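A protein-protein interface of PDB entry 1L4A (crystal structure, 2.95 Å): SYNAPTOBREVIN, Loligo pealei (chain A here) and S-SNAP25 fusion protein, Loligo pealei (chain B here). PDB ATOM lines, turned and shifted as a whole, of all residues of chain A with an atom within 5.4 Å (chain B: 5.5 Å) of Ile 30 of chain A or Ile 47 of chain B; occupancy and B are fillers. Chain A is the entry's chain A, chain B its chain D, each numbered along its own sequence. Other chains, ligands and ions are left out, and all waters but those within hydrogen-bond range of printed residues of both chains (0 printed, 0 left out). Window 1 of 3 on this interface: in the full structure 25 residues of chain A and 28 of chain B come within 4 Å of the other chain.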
ATOM      1  N   GLU A  25      23.870 -29.220  10.192  1.00  0.00           N
ATOM      2  CA  GLU A  25      25.269 -28.853  10.153  1.00  0.00           C
ATOM      3  C   GLU A  25      25.924 -29.250   8.835  1.00  0.00           C
ATOM      4  O   GLU A  25      26.769 -28.512   8.308  1.00  0.00           O
ATOM      5  CB  GLU A  25      25.991 -29.447  11.355  1.00  0.00           C
ATOM      6  CG  GLU A  25      25.395 -28.920  12.639  1.00  0.00           C
ATOM      7  CD  GLU A  25      26.355 -28.953  13.805  1.00  0.00           C
ATOM      8  OE1 GLU A  25      26.625 -30.053  14.348  1.00  0.00           O
ATOM      9  OE2 GLU A  25      26.845 -27.864  14.180  1.00  0.00           O
ATOM     10  N   GLU A  26      25.534 -30.388   8.271  1.00  0.00           N
ATOM     11  CA  GLU A  26      26.129 -30.749   7.000  1.00  0.00           C
ATOM     12  C   GLU A  26      25.798 -29.663   6.002  1.00  0.00           C
ATOM     13  O   GLU A  26      26.649 -29.243   5.229  1.00  0.00           O
ATOM     14  CB  GLU A  26      25.591 -32.058   6.444  1.00  0.00           C
ATOM     15  CG  GLU A  26      26.075 -32.240   5.005  1.00  0.00           C
ATOM     16  CD  GLU A  26      25.394 -33.367   4.277  1.00  0.00           C
ATOM     17  OE1 GLU A  26      24.161 -33.505   4.457  1.00  0.00           O
ATOM     18  OE2 GLU A  26      26.092 -34.097   3.525  1.00  0.00           O
ATOM     19  N   VAL A  27      24.546 -29.220   6.010  1.00  0.00           N
ATOM     20  CA  VAL A  27      24.123 -28.180   5.081  1.00  0.00           C
ATOM     21  C   VAL A  27      24.905 -26.920   5.326  1.00  0.00           C
ATOM     22  O   VAL A  27      25.154 -26.158   4.404  1.00  0.00           O
ATOM     23  CB  VAL A  27      22.629 -27.830   5.212  1.00  0.00           C
ATOM     24  CG1 VAL A  27      22.264 -26.818   4.130  1.00  0.00           C
ATOM     25  CG2 VAL A  27      21.773 -29.087   5.093  1.00  0.00           C
ATOM     26  N   VAL A  28      25.292 -26.695   6.572  1.00  0.00           N
ATOM     27  CA  VAL A  28      26.053 -25.502   6.865  1.00  0.00           C
ATOM     28  C   VAL A  28      27.359 -25.562   6.101  1.00  0.00           C
ATOM     29  O   VAL A  28      27.749 -24.589   5.468  1.00  0.00           O
ATOM     30  CB  VAL A  28      26.372 -25.362   8.348  1.00  0.00           C
ATOM     31  CG1 VAL A  28      26.959 -23.973   8.607  1.00  0.00           C
ATOM     32  CG2 VAL A  28      25.119 -25.575   9.175  1.00  0.00           C
ATOM     33  N   ASP A  29      28.032 -26.708   6.151  1.00  0.00           N
ATOM     34  CA  ASP A  29      29.298 -26.872   5.444  1.00  0.00           C
ATOM     35  C   ASP A  29      29.146 -26.798   3.944  1.00  0.00           C
ATOM     36  O   ASP A  29      29.957 -26.168   3.270  1.00  0.00           O
ATOM     37  CB  ASP A  29      29.961 -28.175   5.845  1.00  0.00           C
ATOM     38  CG  ASP A  29      30.662 -28.060   7.184  1.00  0.00           C
ATOM     39  OD1 ASP A  29      31.507 -27.137   7.324  1.00  0.00           O
ATOM     40  OD2 ASP A  29      30.370 -28.875   8.092  1.00  0.00           O
ATOM     41  N   ILE A  30      28.120 -27.433   3.402  1.00  0.00           N
ATOM     42  CA  ILE A  30      27.921 -27.336   1.972  1.00  0.00           C
ATOM     43  C   ILE A  30      27.845 -25.853   1.617  1.00  0.00           C
ATOM     44  O   ILE A  30      28.199 -25.458   0.512  1.00  0.00           O
ATOM     45  CB  ILE A  30      26.620 -28.002   1.533  1.00  0.00           C
ATOM     46  CG1 ILE A  30      26.630 -29.471   1.941  1.00  0.00           C
ATOM     47  CG2 ILE A  30      26.439 -27.828   0.037  1.00  0.00           C
ATOM     48  CD1 ILE A  30      25.441 -30.241   1.449  1.00  0.00           C
ATOM     49  N   MET A  31      27.382 -25.032   2.562  1.00  0.00           N
ATOM     50  CA  MET A  31      27.266 -23.589   2.327  1.00  0.00           C
ATOM     51  C   MET A  31      28.547 -22.791   2.557  1.00  0.00           C
ATOM     52  O   MET A  31      28.692 -21.709   1.988  1.00  0.00           O
ATOM     53  CB  MET A  31      26.150 -22.987   3.175  1.00  0.00           C
ATOM     54  CG  MET A  31      24.771 -23.387   2.729  1.00  0.00           C
ATOM     55  SD  MET A  31      24.379 -22.729   1.126  1.00  0.00           S
ATOM     56  CE  MET A  31      23.711 -21.117   1.576  1.00  0.00           C
ATOM     57  N   ARG A  32      29.456 -23.293   3.398  1.00  0.00           N
ATOM     58  CA  ARG A  32      30.727 -22.598   3.629  1.00  0.00           C
ATOM     59  C   ARG A  32      31.458 -22.660   2.307  1.00  0.00           C
ATOM     60  O   ARG A  32      32.216 -21.766   1.955  1.00  0.00           O
ATOM     61  CB  ARG A  32      31.597 -23.297   4.677  1.00  0.00           C
ATOM     62  CG  ARG A  32      31.192 -23.083   6.120  1.00  0.00           C
ATOM     63  CD  ARG A  32      32.340 -23.422   7.072  1.00  0.00           C
ATOM     64  NE  ARG A  32      31.951 -23.240   8.467  1.00  0.00           N
ATOM     65  CZ  ARG A  32      31.597 -22.073   9.005  1.00  0.00           C
ATOM     66  NH1 ARG A  32      31.585 -20.970   8.272  1.00  0.00           N
ATOM     67  NH2 ARG A  32      31.237 -22.010  10.280  1.00  0.00           N
ATOM     68  N   VAL A  33      31.212 -23.747   1.585  1.00  0.00           N
ATOM     69  CA  VAL A  33      31.818 -23.978   0.289  1.00  0.00           C
ATOM     70  C   VAL A  33      31.193 -23.057  -0.745  1.00  0.00           C
ATOM     71  O   VAL A  33      31.892 -22.451  -1.553  1.00  0.00           O
ATOM     72  CB  VAL A  33      31.621 -25.444  -0.130  1.00  0.00           C
ATOM     73  CG1 VAL A  33      31.956 -25.625  -1.594  1.00  0.00           C
ATOM     74  CG2 VAL A  33      32.490 -26.344   0.742  1.00  0.00           C
ATOM     75  N   ASN A  34      29.871 -22.942  -0.712  1.00  0.00           N
ATOM     76  CA  ASN A  34      29.159 -22.084  -1.658  1.00  0.00           C
ATOM     77  C   ASN A  34      29.471 -20.610  -1.470  1.00  0.00           C
ATOM     78  O   ASN A  34      29.599 -19.884  -2.444  1.00  0.00           O
ATOM     79  CB  ASN A  34      27.653 -22.311  -1.544  1.00  0.00           C
ATOM     80  CG  ASN A  34      27.244 -23.696  -1.991  1.00  0.00           C
ATOM     81  OD1 ASN A  34      28.093 -24.535  -2.294  1.00  0.00           O
ATOM     82  ND2 ASN A  34      25.940 -23.944  -2.042  1.00  0.00           N
ATOM     83  N   LEU B  42      16.656 -27.454   2.009  1.00  0.00           N
ATOM     84  CA  LEU B  42      17.646 -26.406   1.805  1.00  0.00           C
ATOM     85  C   LEU B  42      18.910 -27.064   1.295  1.00  0.00           C
ATOM     86  O   LEU B  42      19.736 -26.417   0.653  1.00  0.00           O
ATOM     87  CB  LEU B  42      17.954 -25.656   3.104  1.00  0.00           C
ATOM     88  CG  LEU B  42      17.141 -24.390   3.377  1.00  0.00           C
ATOM     89  CD1 LEU B  42      15.663 -24.704   3.315  1.00  0.00           C
ATOM     90  CD2 LEU B  42      17.510 -23.845   4.738  1.00  0.00           C
ATOM     91  N   ARG B  43      19.067 -28.354   1.579  1.00  0.00           N
ATOM     92  CA  ARG B  43      20.241 -29.065   1.109  1.00  0.00           C
ATOM     93  C   ARG B  43      20.277 -29.050  -0.414  1.00  0.00           C
ATOM     94  O   ARG B  43      21.191 -28.475  -1.005  1.00  0.00           O
ATOM     95  CB  ARG B  43      20.233 -30.503   1.593  1.00  0.00           C
ATOM     96  CG  ARG B  43      21.556 -31.205   1.352  1.00  0.00           C
ATOM     97  CD  ARG B  43      21.582 -32.588   1.975  1.00  0.00           C
ATOM     98  NE  ARG B  43      22.928 -33.150   1.983  1.00  0.00           N
ATOM     99  CZ  ARG B  43      23.587 -33.544   0.898  1.00  0.00           C
ATOM    100  NH1 ARG B  43      23.026 -33.444  -0.302  1.00  0.00           N
ATOM    101  NH2 ARG B  43      24.817 -34.035   1.013  1.00  0.00           N
ATOM    102  N   ASN B  44      19.283 -29.670  -1.048  1.00  0.00           N
ATOM    103  CA  ASN B  44      19.234 -29.706  -2.506  1.00  0.00           C
ATOM    104  C   ASN B  44      19.587 -28.351  -3.078  1.00  0.00           C
ATOM    105  O   ASN B  44      20.332 -28.273  -4.040  1.00  0.00           O
ATOM    106  CB  ASN B  44      17.851 -30.101  -3.014  1.00  0.00           C
ATOM    107  CG  ASN B  44      17.368 -31.419  -2.442  1.00  0.00           C
ATOM    108  OD1 ASN B  44      18.154 -32.341  -2.201  1.00  0.00           O
ATOM    109  ND2 ASN B  44      16.060 -31.521  -2.239  1.00  0.00           N
ATOM    110  N   MET B  45      19.045 -27.283  -2.493  1.00  0.00           N
ATOM    111  CA  MET B  45      19.338 -25.930  -2.965  1.00  0.00           C
ATOM    112  C   MET B  45      20.818 -25.617  -2.765  1.00  0.00           C
ATOM    113  O   MET B  45      21.468 -25.070  -3.652  1.00  0.00           O
ATOM    114  CB  MET B  45      18.496 -24.889  -2.220  1.00  0.00           C
ATOM    115  CG  MET B  45      17.073 -24.717  -2.730  1.00  0.00           C
ATOM    116  SD  MET B  45      16.176 -23.321  -1.938  1.00  0.00           S
ATOM    117  CE  MET B  45      14.830 -24.199  -1.184  1.00  0.00           C
ATOM    118  N   ALA B  46      21.350 -25.969  -1.598  1.00  0.00           N
ATOM    119  CA  ALA B  46      22.759 -25.728  -1.301  1.00  0.00           C
ATOM    120  C   ALA B  46      23.644 -26.490  -2.303  1.00  0.00           C
ATOM    121  O   ALA B  46      24.654 -25.969  -2.784  1.00  0.00           O
ATOM    122  CB  ALA B  46      23.074 -26.151   0.143  1.00  0.00           C
ATOM    123  N   ILE B  47      23.258 -27.720  -2.623  1.00  0.00           N
ATOM    124  CA  ILE B  47      24.011 -28.508  -3.587  1.00  0.00           C
ATOM    125  C   ILE B  47      23.835 -27.888  -4.982  1.00  0.00           C
ATOM    126  O   ILE B  47      24.803 -27.714  -5.716  1.00  0.00           O
ATOM    127  CB  ILE B  47      23.531 -29.978  -3.630  1.00  0.00           C
ATOM    128  CG1 ILE B  47      23.609 -30.614  -2.236  1.00  0.00           C
ATOM    129  CG2 ILE B  47      24.401 -30.762  -4.595  1.00  0.00           C
ATOM    130  CD1 ILE B  47      25.010 -31.006  -1.797  1.00  0.00           C
ATOM    131  N   ASP B  48      22.604 -27.555  -5.352  1.00  0.00           N
ATOM    132  CA  ASP B  48      22.374 -26.946  -6.654  1.00  0.00           C
ATOM    133  C   ASP B  48      23.284 -25.738  -6.784  1.00  0.00           C
ATOM    134  O   ASP B  48      24.372 -25.846  -7.341  1.00  0.00           O
ATOM    135  CB  ASP B  48      20.915 -26.499  -6.819  1.00  0.00           C
ATOM    136  CG  ASP B  48      19.968 -27.662  -7.081  1.00  0.00           C
ATOM    137  OD1 ASP B  48      20.170 -28.389  -8.075  1.00  0.00           O
ATOM    138  OD2 ASP B  48      19.014 -27.850  -6.296  1.00  0.00           O
ATOM    139  N   MET B  49      22.848 -24.597  -6.254  1.00  0.00           N
ATOM    140  CA  MET B  49      23.626 -23.360  -6.318  1.00  0.00           C
ATOM    141  C   MET B  49      25.123 -23.627  -6.204  1.00  0.00           C
ATOM    142  O   MET B  49      25.915 -23.066  -6.952  1.00  0.00           O
ATOM    143  CB  MET B  49      23.185 -22.402  -5.204  1.00  0.00           C
ATOM    144  CG  MET B  49      23.940 -22.541  -3.876  1.00  0.00           C
ATOM    145  SD  MET B  49      23.074 -21.774  -2.463  1.00  0.00           S
ATOM    146  CE  MET B  49      22.457 -20.278  -3.178  1.00  0.00           C
ATOM    147  N   GLY B  50      25.501 -24.491  -5.267  1.00  0.00           N
ATOM    148  CA  GLY B  50      26.903 -24.825  -5.086  1.00  0.00           C
ATOM    149  C   GLY B  50      27.537 -25.292  -6.384  1.00  0.00           C
ATOM    150  O   GLY B  50      28.636 -24.865  -6.750  1.00  0.00           O
ATOM    151  N   ASN B  51      26.846 -26.184  -7.084  1.00  0.00           N
ATOM    152  CA  ASN B  51      27.353 -26.682  -8.350  1.00  0.00           C
ATOM    153  C   ASN B  51      27.327 -25.562  -9.386  1.00  0.00           C
ATOM    154  O   ASN B  51      28.313 -25.368 -10.100  1.00  0.00           O
ATOM    155  CB  ASN B  51      26.538 -27.894  -8.828  1.00  0.00           C
ATOM    156  CG  ASN B  51      26.861 -29.174  -8.041  1.00  0.00           C
ATOM    157  OD1 ASN B  51      26.156 -30.186  -8.152  1.00  0.00           O
ATOM    158  ND2 ASN B  51      27.933 -29.130  -7.251  1.00  0.00           N
ATOM    159  N   GLU B  52      26.226 -24.812  -9.460  1.00  0.00           N
ATOM    160  CA  GLU B  52      26.133 -23.708 -10.423  1.00  0.00           C
ATOM    161  C   GLU B  52      27.206 -22.645 -10.209  1.00  0.00           C
ATOM    162  O   GLU B  52      27.765 -22.122 -11.166  1.00  0.00           O
ATOM    163  CB  GLU B  52      24.760 -23.033 -10.376  1.00  0.00           C
ATOM    164  CG  GLU B  52      23.690 -23.746 -11.184  1.00  0.00           C
ATOM    165  CD  GLU B  52      22.490 -22.860 -11.473  1.00  0.00           C
ATOM    166  OE1 GLU B  52      22.656 -21.865 -12.212  1.00  0.00           O
ATOM    167  OE2 GLU B  52      21.387 -23.156 -10.962  1.00  0.00           O
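The side-chain amide nitrogen of Asn 34 of chain A lies within hydrogen-bond range of the backbone carbonyl oxygen of Ala 46 of chain B (2.5 Å).
SD of Met 49 of chain B lies close to ND2 of Asn 34 of chain A (3.6 Å).
NE of Arg 43 of chain B is in salt-bridge range of OE1 of Glu 26 of chain A (2.8 Å).
The side-chain amide nitrogen of Asn 34 of chain A lies close to the backbone NH of Gly 50 of chain B.
The side-chain amide oxygen (OD1) of Asn 34 of chain A sits close to the backbone carbonyl oxygen (O) of Ile 30 of chain A (3.0 Å).
ND2 of Asn 34 of chain A lies within hydrogen-bond range of SD of Met 31 of chain A, 3.7 Å away.
Arg 43 of chain B touches Ile 30 of chain A.
Ala 46 of chain B touches Ile 30 of chain A.
Ile 30 of chain A touches Ile 47 of chain B.
CB of Ala 46 of chain B touches SD of Met 31 of chain A, at 3.8 Å.
Met 49 of chain B touches Met 31 of chain A.
Printed residues of chain B within 4 Å of Glu 26 of chain A: Arg 43.
Ile 30 of chain A touches just these residues of chain B: Arg 43 (3.8 Å), Ala 46 (3.8 Å) and Ile 47 (3.4 Å).
Of the printed residues of chain B, Asn 34 of chain A touches Ala 46, Met 49 and Gly 50.
Leu 42 of chain B touches none of the printed residues of chain A.
Of the printed residues of chain A, Arg 43 of chain B touches Glu 26 (2.8 Å) and Ile 30 (3.8 Å).
Printed residues of chain A within 4 Å of Ala 46 of chain B: Ile 30 (3.8 Å), Met 31 (3.8 Å) and Asn 34 (2.5 Å).
Ile 47 of chain B touches just one residue of chain A: Ile 30.
Glu 52 of chain B touches none of the printed residues of chain A.
The nearest residue of chain A that does not touch Ile 47 of chain B is Asn 34 of chain A (4.7 Å).
Hydrophobic or aromatic side chains of chain A that line the printed part of chain B: Ile 30 and Met 31.
Printed residues of chain B that touch a printed residue of chain A: Arg 43, Ala 46, Ile 47, Met 49 and Gly 50.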
